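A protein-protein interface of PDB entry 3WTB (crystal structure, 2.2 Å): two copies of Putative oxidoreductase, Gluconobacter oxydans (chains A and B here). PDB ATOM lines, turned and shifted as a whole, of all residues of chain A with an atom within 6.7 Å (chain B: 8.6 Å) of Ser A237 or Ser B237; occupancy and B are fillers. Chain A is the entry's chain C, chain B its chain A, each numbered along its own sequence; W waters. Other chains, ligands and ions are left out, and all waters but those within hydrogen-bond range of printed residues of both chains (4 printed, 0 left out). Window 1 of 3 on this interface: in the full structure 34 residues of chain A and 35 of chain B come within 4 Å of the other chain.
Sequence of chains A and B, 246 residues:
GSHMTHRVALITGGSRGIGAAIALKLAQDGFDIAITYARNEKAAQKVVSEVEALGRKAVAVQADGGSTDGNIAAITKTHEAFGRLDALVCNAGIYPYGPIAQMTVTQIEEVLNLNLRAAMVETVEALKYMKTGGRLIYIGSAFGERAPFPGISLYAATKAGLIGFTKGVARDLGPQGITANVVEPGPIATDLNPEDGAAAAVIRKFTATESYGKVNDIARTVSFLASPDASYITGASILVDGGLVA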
ATOM      1  N   GLU A 145     -13.811 -15.051  35.658  1.00  0.00           N
ATOM      2  CA  GLU A 145     -12.815 -15.924  36.270  1.00  0.00           C
ATOM      3  C   GLU A 145     -12.117 -15.248  37.413  1.00  0.00           C
ATOM      4  O   GLU A 145     -11.529 -15.934  38.233  1.00  0.00           O
ATOM      5  CB  GLU A 145     -11.742 -16.375  35.239  1.00  0.00           C
ATOM      6  CG  GLU A 145     -12.246 -17.370  34.196  1.00  0.00           C
ATOM      7  CD  GLU A 145     -11.138 -18.159  33.500  1.00  0.00           C
ATOM      8  OE1 GLU A 145     -10.281 -18.738  34.204  1.00  0.00           O
ATOM      9  OE2 GLU A 145     -11.121 -18.197  32.255  1.00  0.00           O
ATOM     10  N   ILE A 163     -19.722 -19.651  31.364  1.00  0.00           N
ATOM     11  CA  ILE A 163     -18.659 -20.650  31.263  1.00  0.00           C
ATOM     12  C   ILE A 163     -19.272 -22.011  31.487  1.00  0.00           C
ATOM     13  O   ILE A 163     -18.975 -22.975  30.772  1.00  0.00           O
ATOM     14  CB  ILE A 163     -17.530 -20.422  32.287  1.00  0.00           C
ATOM     15  CG1 ILE A 163     -16.862 -19.080  32.047  1.00  0.00           C
ATOM     16  CG2 ILE A 163     -16.460 -21.559  32.232  1.00  0.00           C
ATOM     17  CD1 ILE A 163     -15.884 -18.745  33.167  1.00  0.00           C
ATOM     18  N   THR A 166     -21.515 -23.008  28.561  1.00  0.00           N
ATOM     19  CA  THR A 166     -20.669 -23.404  27.450  1.00  0.00           C
ATOM     20  C   THR A 166     -20.202 -24.860  27.598  1.00  0.00           C
ATOM     21  O   THR A 166     -20.206 -25.634  26.638  1.00  0.00           O
ATOM     22  CB  THR A 166     -19.448 -22.445  27.337  1.00  0.00           C
ATOM     23  OG1 THR A 166     -19.905 -21.139  26.982  1.00  0.00           O
ATOM     24  CG2 THR A 166     -18.468 -22.895  26.255  1.00  0.00           C
ATOM     25  N   LYS A 167     -19.780 -25.210  28.796  1.00  0.00           N
ATOM     26  CA  LYS A 167     -19.289 -26.545  29.039  1.00  0.00           C
ATOM     27  C   LYS A 167     -20.415 -27.563  28.819  1.00  0.00           C
ATOM     28  O   LYS A 167     -20.197 -28.609  28.215  1.00  0.00           O
ATOM     29  CB  LYS A 167     -18.710 -26.661  30.442  1.00  0.00           C
ATOM     30  CG  LYS A 167     -17.339 -26.015  30.610  1.00  0.00           C
ATOM     31  CD  LYS A 167     -16.900 -25.884  32.065  1.00  0.00           C
ATOM     32  CE  LYS A 167     -15.460 -25.359  32.101  1.00  0.00           C
ATOM     33  NZ  LYS A 167     -14.797 -25.039  33.417  1.00  0.00           N
ATOM     34  N   ASN A 181     -18.103 -22.429  22.560  1.00  0.00           N
ATOM     35  CA  ASN A 181     -16.901 -21.875  23.169  1.00  0.00           C
ATOM     36  C   ASN A 181     -17.182 -20.454  23.685  1.00  0.00           C
ATOM     37  O   ASN A 181     -18.103 -19.804  23.211  1.00  0.00           O
ATOM     38  CB  ASN A 181     -15.796 -21.775  22.109  1.00  0.00           C
ATOM     39  CG  ASN A 181     -15.348 -23.120  21.582  1.00  0.00           C
ATOM     40  OD1 ASN A 181     -15.483 -23.464  20.360  1.00  0.00           O
ATOM     41  ND2 ASN A 181     -14.803 -23.883  22.467  1.00  0.00           N
ATOM     42  N   VAL A 182     -16.380 -19.997  24.659  1.00  0.00           N
ATOM     43  CA  VAL A 182     -16.532 -18.659  25.236  1.00  0.00           C
ATOM     44  C   VAL A 182     -15.272 -17.856  25.066  1.00  0.00           C
ATOM     45  O   VAL A 182     -14.191 -18.332  25.393  1.00  0.00           O
ATOM     46  CB  VAL A 182     -16.710 -18.638  26.764  1.00  0.00           C
ATOM     47  CG1 VAL A 182     -17.413 -17.372  27.272  1.00  0.00           C
ATOM     48  CG2 VAL A 182     -17.400 -19.837  27.224  1.00  0.00           C
ATOM     49  N   VAL A 183     -15.413 -16.645  24.569  1.00  0.00           N
ATOM     50  CA  VAL A 183     -14.347 -15.688  24.527  1.00  0.00           C
ATOM     51  C   VAL A 183     -14.504 -14.763  25.718  1.00  0.00           C
ATOM     52  O   VAL A 183     -15.607 -14.290  25.973  1.00  0.00           O
ATOM     53  CB  VAL A 183     -14.392 -14.853  23.258  1.00  0.00           C
ATOM     54  CG1 VAL A 183     -13.205 -13.880  23.222  1.00  0.00           C
ATOM     55  CG2 VAL A 183     -14.366 -15.754  22.053  1.00  0.00           C
ATOM     56  N   GLU A 184     -13.417 -14.507  26.442  1.00  0.00           N
ATOM     57  CA  GLU A 184     -13.440 -13.752  27.705  1.00  0.00           C
ATOM     58  C   GLU A 184     -12.583 -12.494  27.638  1.00  0.00           C
ATOM     59  O   GLU A 184     -11.404 -12.495  28.016  1.00  0.00           O
ATOM     60  CB  GLU A 184     -12.952 -14.648  28.832  1.00  0.00           C
ATOM     61  CG  GLU A 184     -13.859 -15.857  29.045  1.00  0.00           C
ATOM     62  CD  GLU A 184     -13.425 -16.725  30.203  1.00  0.00           C
ATOM     63  OE1 GLU A 184     -12.225 -17.130  30.226  1.00  0.00           O
ATOM     64  OE2 GLU A 184     -14.261 -16.950  31.116  1.00  0.00           O
ATOM     65  N   ILE A 233     -12.167 -27.681  18.787  1.00  0.00           N
ATOM     66  CA  ILE A 233     -12.198 -26.767  19.899  1.00  0.00           C
ATOM     67  C   ILE A 233     -13.641 -26.672  20.356  1.00  0.00           C
ATOM     68  O   ILE A 233     -14.474 -26.070  19.686  1.00  0.00           O
ATOM     69  CB  ILE A 233     -11.722 -25.303  19.576  1.00  0.00           C
ATOM     70  CG1 ILE A 233     -10.561 -25.139  18.612  1.00  0.00           C
ATOM     71  CG2 ILE A 233     -11.681 -24.486  20.847  1.00  0.00           C
ATOM     72  CD1 ILE A 233      -9.425 -25.850  19.100  1.00  0.00           C
ATOM     73  N   GLY A 235     -16.047 -26.413  24.249  1.00  0.00           N
ATOM     74  CA  GLY A 235     -15.956 -26.304  25.687  1.00  0.00           C
ATOM     75  C   GLY A 235     -14.890 -25.300  26.155  1.00  0.00           C
ATOM     76  O   GLY A 235     -14.654 -25.159  27.345  1.00  0.00           O
ATOM     77  N   ALA A 236     -14.169 -24.683  25.243  1.00  0.00           N
ATOM     78  CA  ALA A 236     -13.014 -23.876  25.615  1.00  0.00           C
ATOM     79  C   ALA A 236     -13.385 -22.459  26.014  1.00  0.00           C
ATOM     80  O   ALA A 236     -14.426 -21.906  25.587  1.00  0.00           O
ATOM     81  CB  ALA A 236     -12.044 -23.828  24.456  1.00  0.00           C
ATOM     82  N   SER A 237     -12.535 -21.891  26.822  1.00  0.00           N
ATOM     83  CA  SER A 237     -12.581 -20.468  27.122  1.00  0.00           C
ATOM     84  C   SER A 237     -11.271 -19.880  26.684  1.00  0.00           C
ATOM     85  O   SER A 237     -10.211 -20.426  26.955  1.00  0.00           O
ATOM     86  CB  SER A 237     -12.868 -20.216  28.607  1.00  0.00           C
ATOM     87  OG  SER A 237     -12.027 -20.979  29.405  1.00  0.00           O
ATOM     88  N   ILE A 238     -11.342 -18.750  25.985  1.00  0.00           N
ATOM     89  CA  ILE A 238     -10.169 -18.015  25.610  1.00  0.00           C
ATOM     90  C   ILE A 238     -10.171 -16.619  26.260  1.00  0.00           C
ATOM     91  O   ILE A 238     -10.920 -15.751  25.852  1.00  0.00           O
ATOM     92  CB  ILE A 238     -10.051 -17.911  24.101  1.00  0.00           C
ATOM     93  CG1 ILE A 238     -10.054 -19.320  23.479  1.00  0.00           C
ATOM     94  CG2 ILE A 238      -8.751 -17.213  23.714  1.00  0.00           C
ATOM     95  CD1 ILE A 238      -9.813 -19.327  21.986  1.00  0.00           C
ATOM     96  N   LEU A 239      -9.211 -16.410  27.158  1.00  0.00           N
ATOM     97  CA  LEU A 239      -8.986 -15.118  27.796  1.00  0.00           C
ATOM     98  C   LEU A 239      -8.251 -14.200  26.843  1.00  0.00           C
ATOM     99  O   LEU A 239      -7.213 -14.572  26.283  1.00  0.00           O
ATOM    100  CB  LEU A 239      -8.155 -15.302  29.029  1.00  0.00           C
ATOM    101  CG  LEU A 239      -8.811 -15.931  30.242  1.00  0.00           C
ATOM    102  CD1 LEU A 239      -7.788 -16.441  31.233  1.00  0.00           C
ATOM    103  CD2 LEU A 239      -9.716 -14.887  30.870  1.00  0.00           C
ATOM    104  N   TYR B 138       3.706 -22.673  25.489  1.00  0.00           N
ATOM    105  CA  TYR B 138       3.973 -23.948  26.109  1.00  0.00           C
ATOM    106  C   TYR B 138       2.859 -24.941  25.645  1.00  0.00           C
ATOM    107  O   TYR B 138       1.658 -24.566  25.592  1.00  0.00           O
ATOM    108  CB  TYR B 138       3.952 -23.776  27.632  1.00  0.00           C
ATOM    109  CG  TYR B 138       4.915 -22.704  28.096  1.00  0.00           C
ATOM    110  CD1 TYR B 138       6.275 -22.992  28.250  1.00  0.00           C
ATOM    111  CD2 TYR B 138       4.497 -21.417  28.291  1.00  0.00           C
ATOM    112  CE1 TYR B 138       7.196 -22.036  28.628  1.00  0.00           C
ATOM    113  CE2 TYR B 138       5.412 -20.421  28.638  1.00  0.00           C
ATOM    114  CZ  TYR B 138       6.752 -20.718  28.799  1.00  0.00           C
ATOM    115  OH  TYR B 138       7.639 -19.726  29.153  1.00  0.00           O
ATOM    116  N   GLY B 140       0.908 -27.736  26.839  1.00  0.00           N
ATOM    117  CA  GLY B 140       0.455 -28.398  28.020  1.00  0.00           C
ATOM    118  C   GLY B 140      -0.381 -29.590  27.603  1.00  0.00           C
ATOM    119  O   GLY B 140       0.017 -30.348  26.752  1.00  0.00           O
ATOM    120  N   SER B 141      -1.478 -29.798  28.294  1.00  0.00           N
ATOM    121  CA  SER B 141      -2.407 -30.885  27.994  1.00  0.00           C
ATOM    122  C   SER B 141      -3.734 -30.573  28.656  1.00  0.00           C
ATOM    123  O   SER B 141      -3.785 -30.005  29.773  1.00  0.00           O
ATOM    124  CB  SER B 141      -1.896 -32.193  28.588  1.00  0.00           C
ATOM    125  OG  SER B 141      -2.852 -33.251  28.473  1.00  0.00           O
ATOM    126  N   GLU B 145      -5.888 -30.122  33.363  1.00  0.00           N
ATOM    127  CA  GLU B 145      -7.081 -29.578  33.971  1.00  0.00           C
ATOM    128  C   GLU B 145      -8.054 -30.638  34.414  1.00  0.00           C
ATOM    129  O   GLU B 145      -8.888 -30.370  35.264  1.00  0.00           O
ATOM    130  CB  GLU B 145      -7.819 -28.650  32.984  1.00  0.00           C
ATOM    131  CG  GLU B 145      -7.097 -27.358  32.703  1.00  0.00           C
ATOM    132  CD  GLU B 145      -8.034 -26.273  32.130  1.00  0.00           C
ATOM    133  OE1 GLU B 145      -9.104 -25.999  32.730  1.00  0.00           O
ATOM    134  OE2 GLU B 145      -7.673 -25.661  31.101  1.00  0.00           O
ATOM    135  N   LYS B 159       1.801 -30.988  33.630  1.00  0.00           N
ATOM    136  CA  LYS B 159       1.052 -30.165  32.768  1.00  0.00           C
ATOM    137  C   LYS B 159       0.281 -29.078  33.505  1.00  0.00           C
ATOM    138  O   LYS B 159       0.101 -27.975  32.960  1.00  0.00           O
ATOM    139  CB  LYS B 159       0.126 -31.001  31.856  1.00  0.00           C
ATOM    140  CG  LYS B 159       0.853 -31.901  30.900  1.00  0.00           C
ATOM    141  CD  LYS B 159       2.001 -31.231  30.147  1.00  0.00           C
ATOM    142  CE  LYS B 159       2.439 -32.043  28.926  1.00  0.00           C
ATOM    143  NZ  LYS B 159       3.314 -31.281  28.046  1.00  0.00           N
ATOM    144  N   LEU B 162       2.741 -26.279  34.160  1.00  0.00           N
ATOM    145  CA  LEU B 162       2.926 -25.366  33.077  1.00  0.00           C
ATOM    146  C   LEU B 162       1.867 -24.284  33.057  1.00  0.00           C
ATOM    147  O   LEU B 162       2.162 -23.174  32.620  1.00  0.00           O
ATOM    148  CB  LEU B 162       2.842 -26.053  31.731  1.00  0.00           C
ATOM    149  CG  LEU B 162       4.030 -26.862  31.268  1.00  0.00           C
ATOM    150  CD1 LEU B 162       3.679 -27.563  29.973  1.00  0.00           C
ATOM    151  CD2 LEU B 162       5.252 -25.957  31.101  1.00  0.00           C
ATOM    152  N   ILE B 163       0.673 -24.568  33.562  1.00  0.00           N
ATOM    153  CA  ILE B 163      -0.360 -23.529  33.631  1.00  0.00           C
ATOM    154  C   ILE B 163       0.071 -22.433  34.615  1.00  0.00           C
ATOM    155  O   ILE B 163      -0.056 -21.255  34.330  1.00  0.00           O
ATOM    156  CB  ILE B 163      -1.709 -24.095  34.051  1.00  0.00           C
ATOM    157  CG1 ILE B 163      -2.181 -25.164  33.059  1.00  0.00           C
ATOM    158  CG2 ILE B 163      -2.791 -22.988  34.172  1.00  0.00           C
ATOM    159  CD1 ILE B 163      -3.434 -25.876  33.556  1.00  0.00           C
ATOM    160  N   GLY B 164       0.505 -22.852  35.789  1.00  0.00           N
ATOM    161  CA  GLY B 164       0.957 -21.938  36.791  1.00  0.00           C
ATOM    162  C   GLY B 164       2.181 -21.169  36.303  1.00  0.00           C
ATOM    163  O   GLY B 164       2.285 -19.937  36.557  1.00  0.00           O
ATOM    164  N   THR B 166       3.020 -20.434  33.214  1.00  0.00           N
ATOM    165  CA  THR B 166       2.510 -19.512  32.205  1.00  0.00           C
ATOM    166  C   THR B 166       1.903 -18.268  32.803  1.00  0.00           C
ATOM    167  O   THR B 166       2.146 -17.131  32.345  1.00  0.00           O
ATOM    168  CB  THR B 166       1.485 -20.233  31.315  1.00  0.00           C
ATOM    169  OG1 THR B 166       2.108 -21.273  30.599  1.00  0.00           O
ATOM    170  CG2 THR B 166       0.831 -19.276  30.295  1.00  0.00           C
ATOM    171  N   LYS B 167       1.123 -18.442  33.855  1.00  0.00           N
ATOM    172  CA  LYS B 167       0.489 -17.303  34.536  1.00  0.00           C
ATOM    173  C   LYS B 167       1.497 -16.387  35.162  1.00  0.00           C
ATOM    174  O   LYS B 167       1.425 -15.147  34.990  1.00  0.00           O
ATOM    175  CB  LYS B 167      -0.499 -17.772  35.577  1.00  0.00           C
ATOM    176  CG  LYS B 167      -1.828 -18.372  35.034  1.00  0.00           C
ATOM    177  CD  LYS B 167      -2.519 -19.246  36.132  1.00  0.00           C
ATOM    178  CE  LYS B 167      -3.773 -18.633  36.768  1.00  0.00           C
ATOM    179  NZ  LYS B 167      -4.686 -17.908  35.835  1.00  0.00           N
ATOM    180  N   ALA B 180       3.003 -14.951  27.087  1.00  0.00           N
ATOM    181  CA  ALA B 180       3.171 -16.318  27.468  1.00  0.00           C
ATOM    182  C   ALA B 180       1.772 -16.985  27.587  1.00  0.00           C
ATOM    183  O   ALA B 180       0.921 -16.518  28.308  1.00  0.00           O
ATOM    184  CB  ALA B 180       3.910 -16.398  28.803  1.00  0.00           C
ATOM    185  N   ASN B 181       1.592 -18.103  26.894  1.00  0.00           N
ATOM    186  CA  ASN B 181       0.322 -18.785  26.811  1.00  0.00           C
ATOM    187  C   ASN B 181       0.550 -20.292  26.738  1.00  0.00           C
ATOM    188  O   ASN B 181       1.608 -20.743  26.300  1.00  0.00           O
ATOM    189  CB  ASN B 181      -0.401 -18.338  25.539  1.00  0.00           C
ATOM    190  CG  ASN B 181      -0.779 -16.851  25.530  1.00  0.00           C
ATOM    191  OD1 ASN B 181      -0.297 -16.019  24.690  1.00  0.00           O
ATOM    192  ND2 ASN B 181      -1.644 -16.519  26.412  1.00  0.00           N
ATOM    193  N   VAL B 182      -0.470 -21.057  27.121  1.00  0.00           N
ATOM    194  CA  VAL B 182      -0.397 -22.493  27.057  1.00  0.00           C
ATOM    195  C   VAL B 182      -1.503 -23.082  26.189  1.00  0.00           C
ATOM    196  O   VAL B 182      -2.686 -22.721  26.321  1.00  0.00           O
ATOM    197  CB  VAL B 182      -0.357 -23.096  28.457  1.00  0.00           C
ATOM    198  CG1 VAL B 182      -1.567 -22.725  29.269  1.00  0.00           C
ATOM    199  CG2 VAL B 182      -0.214 -24.608  28.402  1.00  0.00           C
ATOM    200  N   VAL B 183      -1.118 -23.955  25.260  1.00  0.00           N
ATOM    201  CA  VAL B 183      -2.068 -24.741  24.462  1.00  0.00           C
ATOM    202  C   VAL B 183      -2.211 -26.111  25.134  1.00  0.00           C
ATOM    203  O   VAL B 183      -1.218 -26.708  25.456  1.00  0.00           O
ATOM    204  CB  VAL B 183      -1.581 -24.950  23.043  1.00  0.00           C
ATOM    205  CG1 VAL B 183      -2.637 -25.682  22.224  1.00  0.00           C
ATOM    206  CG2 VAL B 183      -1.320 -23.592  22.401  1.00  0.00           C
ATOM    207  N   GLU B 184      -3.458 -26.549  25.339  1.00  0.00           N
ATOM    208  CA  GLU B 184      -3.774 -27.779  26.031  1.00  0.00           C
ATOM    209  C   GLU B 184      -4.491 -28.824  25.142  1.00  0.00           C
ATOM    210  O   GLU B 184      -5.694 -28.909  25.100  1.00  0.00           O
ATOM    211  CB  GLU B 184      -4.639 -27.464  27.237  1.00  0.00           C
ATOM    212  CG  GLU B 184      -3.936 -26.558  28.222  1.00  0.00           C
ATOM    213  CD  GLU B 184      -4.776 -26.254  29.426  1.00  0.00           C
ATOM    214  OE1 GLU B 184      -5.930 -25.785  29.250  1.00  0.00           O
ATOM    215  OE2 GLU B 184      -4.252 -26.479  30.548  1.00  0.00           O
ATOM    216  N   THR B 221      -3.505 -23.427  16.411  1.00  0.00           N
ATOM    217  CA  THR B 221      -3.712 -22.679  17.649  1.00  0.00           C
ATOM    218  C   THR B 221      -2.414 -21.989  18.055  1.00  0.00           C
ATOM    219  O   THR B 221      -2.413 -20.823  18.492  1.00  0.00           O
ATOM    220  CB  THR B 221      -4.192 -23.605  18.764  1.00  0.00           C
ATOM    221  OG1 THR B 221      -5.383 -24.317  18.324  1.00  0.00           O
ATOM    222  CG2 THR B 221      -4.481 -22.815  20.004  1.00  0.00           C
ATOM    223  N   LEU B 225      -1.727 -17.840  18.391  1.00  0.00           N
ATOM    224  CA  LEU B 225      -1.058 -17.214  19.492  1.00  0.00           C
ATOM    225  C   LEU B 225       0.265 -16.523  19.134  1.00  0.00           C
ATOM    226  O   LEU B 225       0.642 -15.513  19.747  1.00  0.00           O
ATOM    227  CB  LEU B 225      -0.804 -18.202  20.589  1.00  0.00           C
ATOM    228  CG  LEU B 225      -2.033 -18.757  21.260  1.00  0.00           C
ATOM    229  CD1 LEU B 225      -1.655 -19.907  22.171  1.00  0.00           C
ATOM    230  CD2 LEU B 225      -2.725 -17.683  22.082  1.00  0.00           C
ATOM    231  N   ILE B 233      -3.279 -11.293  24.194  1.00  0.00           N
ATOM    232  CA  ILE B 233      -3.487 -12.592  24.764  1.00  0.00           C
ATOM    233  C   ILE B 233      -2.268 -13.008  25.522  1.00  0.00           C
ATOM    234  O   ILE B 233      -1.245 -13.321  24.938  1.00  0.00           O
ATOM    235  CB  ILE B 233      -3.808 -13.690  23.712  1.00  0.00           C
ATOM    236  CG1 ILE B 233      -4.982 -13.268  22.878  1.00  0.00           C
ATOM    237  CG2 ILE B 233      -4.132 -15.035  24.404  1.00  0.00           C
ATOM    238  CD1 ILE B 233      -5.379 -14.197  21.763  1.00  0.00           C
ATOM    239  N   THR B 234      -2.397 -13.077  26.846  1.00  0.00           N
ATOM    240  CA  THR B 234      -1.304 -13.507  27.654  1.00  0.00           C
ATOM    241  C   THR B 234      -1.805 -14.050  28.949  1.00  0.00           C
ATOM    242  O   THR B 234      -2.773 -13.569  29.502  1.00  0.00           O
ATOM    243  CB  THR B 234      -0.247 -12.387  27.823  1.00  0.00           C
ATOM    244  OG1 THR B 234       0.953 -12.951  28.359  1.00  0.00           O
ATOM    245  CG2 THR B 234      -0.715 -11.281  28.711  1.00  0.00           C
ATOM    246  N   GLY B 235      -1.130 -15.077  29.441  1.00  0.00           N
ATOM    247  CA  GLY B 235      -1.639 -15.839  30.597  1.00  0.00           C
ATOM    248  C   GLY B 235      -2.759 -16.818  30.256  1.00  0.00           C
ATOM    249  O   GLY B 235      -3.298 -17.443  31.103  1.00  0.00           O
ATOM    250  N   ALA B 236      -3.125 -16.920  28.984  1.00  0.00           N
ATOM    251  CA  ALA B 236      -4.244 -17.730  28.571  1.00  0.00           C
ATOM    252  C   ALA B 236      -3.910 -19.213  28.426  1.00  0.00           C
ATOM    253  O   ALA B 236      -2.782 -19.614  28.138  1.00  0.00           O
ATOM    254  CB  ALA B 236      -4.801 -17.218  27.284  1.00  0.00           C
ATOM    255  N   SER B 237      -4.935 -20.017  28.627  1.00  0.00           N
ATOM    256  CA  SER B 237      -4.890 -21.439  28.238  1.00  0.00           C
ATOM    257  C   SER B 237      -5.956 -21.713  27.207  1.00  0.00           C
ATOM    258  O   SER B 237      -7.104 -21.238  27.353  1.00  0.00           O
ATOM    259  CB  SER B 237      -5.059 -22.332  29.466  1.00  0.00           C
ATOM    260  OG  SER B 237      -6.182 -21.966  30.206  1.00  0.00           O
ATOM    261  N   ILE B 238      -5.596 -22.418  26.128  1.00  0.00           N
ATOM    262  CA  ILE B 238      -6.540 -22.804  25.123  1.00  0.00           C
ATOM    263  C   ILE B 238      -6.648 -24.339  25.030  1.00  0.00           C
ATOM    264  O   ILE B 238      -5.743 -25.008  24.557  1.00  0.00           O
ATOM    265  CB  ILE B 238      -6.187 -22.242  23.771  1.00  0.00           C
ATOM    266  CG1 ILE B 238      -6.098 -20.710  23.883  1.00  0.00           C
ATOM    267  CG2 ILE B 238      -7.277 -22.594  22.759  1.00  0.00           C
ATOM    268  CD1 ILE B 238      -5.891 -20.017  22.539  1.00  0.00           C
ATOM    269  N   LEU B 239      -7.785 -24.851  25.465  1.00  0.00           N
ATOM    270  CA  LEU B 239      -8.095 -26.258  25.352  1.00  0.00           C
ATOM    271  C   LEU B 239      -8.428 -26.593  23.885  1.00  0.00           C
ATOM    272  O   LEU B 239      -9.302 -25.980  23.286  1.00  0.00           O
ATOM    273  CB  LEU B 239      -9.326 -26.581  26.208  1.00  0.00           C
ATOM    274  CG  LEU B 239      -9.097 -26.633  27.697  1.00  0.00           C
ATOM    275  CD1 LEU B 239     -10.421 -26.568  28.450  1.00  0.00           C
ATOM    276  CD2 LEU B 239      -8.354 -27.906  28.050  1.00  0.00           C
ATOM    277  N   VAL B 240      -7.743 -27.597  23.347  1.00  0.00           N
ATOM    278  CA  VAL B 240      -8.022 -28.108  22.056  1.00  0.00           C
ATOM    279  C   VAL B 240      -8.185 -29.609  22.254  1.00  0.00           C
ATOM    280  O   VAL B 240      -7.266 -30.391  21.962  1.00  0.00           O
ATOM    281  CB  VAL B 240      -6.904 -27.746  21.066  1.00  0.00           C
ATOM    282  CG1 VAL B 240      -7.313 -28.136  19.633  1.00  0.00           C
ATOM    283  CG2 VAL B 240      -6.671 -26.249  21.056  1.00  0.00           C
ATOM    284  N   ASP B 241      -9.373 -30.005  22.697  1.00  0.00           N
ATOM    285  CA  ASP B 241      -9.564 -31.318  23.303  1.00  0.00           C
ATOM    286  C   ASP B 241     -10.868 -32.021  23.008  1.00  0.00           C
ATOM    287  O   ASP B 241     -11.226 -32.965  23.686  1.00  0.00           O
ATOM    288  CB  ASP B 241      -9.407 -31.191  24.792  1.00  0.00           C
ATOM    289  CG  ASP B 241     -10.628 -30.515  25.464  1.00  0.00           C
ATOM    290  OD1 ASP B 241     -11.428 -29.796  24.775  1.00  0.00           O
ATOM    291  OD2 ASP B 241     -10.747 -30.681  26.702  1.00  0.00           O
ATOM    292  N   VAL B 245     -12.479 -31.747  28.648  1.00  0.00           N
ATOM    293  CA  VAL B 245     -12.511 -31.068  29.946  1.00  0.00           C
ATOM    294  C   VAL B 245     -13.888 -30.462  30.295  1.00  0.00           C
ATOM    295  O   VAL B 245     -14.116 -30.131  31.418  1.00  0.00           O
ATOM    296  CB  VAL B 245     -11.393 -30.009  29.989  1.00  0.00           C
ATOM    297  CG1 VAL B 245     -11.539 -29.046  31.175  1.00  0.00           C
ATOM    298  CG2 VAL B 245     -10.050 -30.711  30.007  1.00  0.00           C
HETATM  299  O   HOH W   1      -5.284 -12.908  27.618  1.00  0.00           O
HETATM  300  O   HOH W   2      -7.928 -18.913  28.311  1.00  0.00           O
HETATM  301  O   HOH W   3      -9.694 -23.219  27.131  1.00  0.00           O
HETATM  302  O   HOH W   4      -7.458 -19.114  34.591  1.00  0.00           O
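Hydrophobic or aromatic side chains of chain B within 4 Å of the printed part of chain A: Ile B233, Ala B236 and Val B240. Among the printed residues, no Asp or Glu carboxylate lies within 4 Å of a Lys or Arg side-chain nitrogen of the other chain.
Ile A233 touches Leu B239, and with the chains exchanged Leu A239 touches Ile B233. Ala A236 touches Leu B239, and with the chains exchanged Leu A239 touches Ala B236. Ser A237 touches its own counterpart, Ser B237. Positions printed for both chains: 145, 163, 166, 167, 181, 182, 183, 184, 233, 235, 236, 237, 238 and 239.
Ser A237 touches one residue of chain B. Ala A236 touches just one residue of chain B: Leu B239. Of the printed residues of chain A, Ala B236 touches Leu A239. Printed residues of chain A within 4 Å of Val B240: Ile A233. Printed residues of chain A within 4 Å of Ile B233: Leu A239. Printed residues of chain B within 4 Å of Ile A233: Leu B239 and Val B240. Val A183 touches none of the printed residues of chain B. The nearest residue of chain A that does not touch Ser B237 is Ile A238 (4.8 Å). The nearest printed residue of chain B that does not touch Ile A233 is Thr B221 (4.4 Å).
O of Ile B233 lies close to OD1 of Asn B181 (2.9 Å). The side-chain amide nitrogen (ND2) of Asn B181 sits close to the backbone NH (N) of Ala B236 (3.0 Å). N of Val B182 lies within hydrogen-bond range of O of Ala B236. N of Val B240 sits at hydrogen-bond distance from O of Glu B184, 3.0 Å away. O of Ile A233 lies close to OD1 of Asn A181. N of Val A182 lies within hydrogen-bond range of O of Ala A236, 2.9 Å away.
Among the printed residues, merely in contact across the chains: Ile A233 with Val B240 (3.2 Å), Leu A239 with Ile B233 (3.6 Å), Ala A236 with Leu B239 (3.7 Å), Leu A239 with Ala B236 (3.7 Å) and Ile A233 with Leu B239 (3.7 Å).
O of Ser A237 lies close to O of Ser B237, 3.2 Å away.
Water W2 lies within hydrogen-bond range of O of Ser B237 (2.6 Å), N of Leu A239 (3.0 Å) and O of Ser A237 (3.1 Å). Water W3 lies within hydrogen-bond range of O of Ser A237 (2.8 Å), N of Leu B239 (3.0 Å) and O of Ser B237 (3.3 Å). Water W4 lies within hydrogen-bond range of the side-chain carboxylate (OE1) of Glu A145 (2.9 Å) and the side-chain amino group (NZ) of Lys B167 (3.3 Å). Water W1 bridges the backbone carbonyl oxygen (O) of Leu A239 (2.9 Å) and the backbone NH (N) of Thr B234 (3.0 Å).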
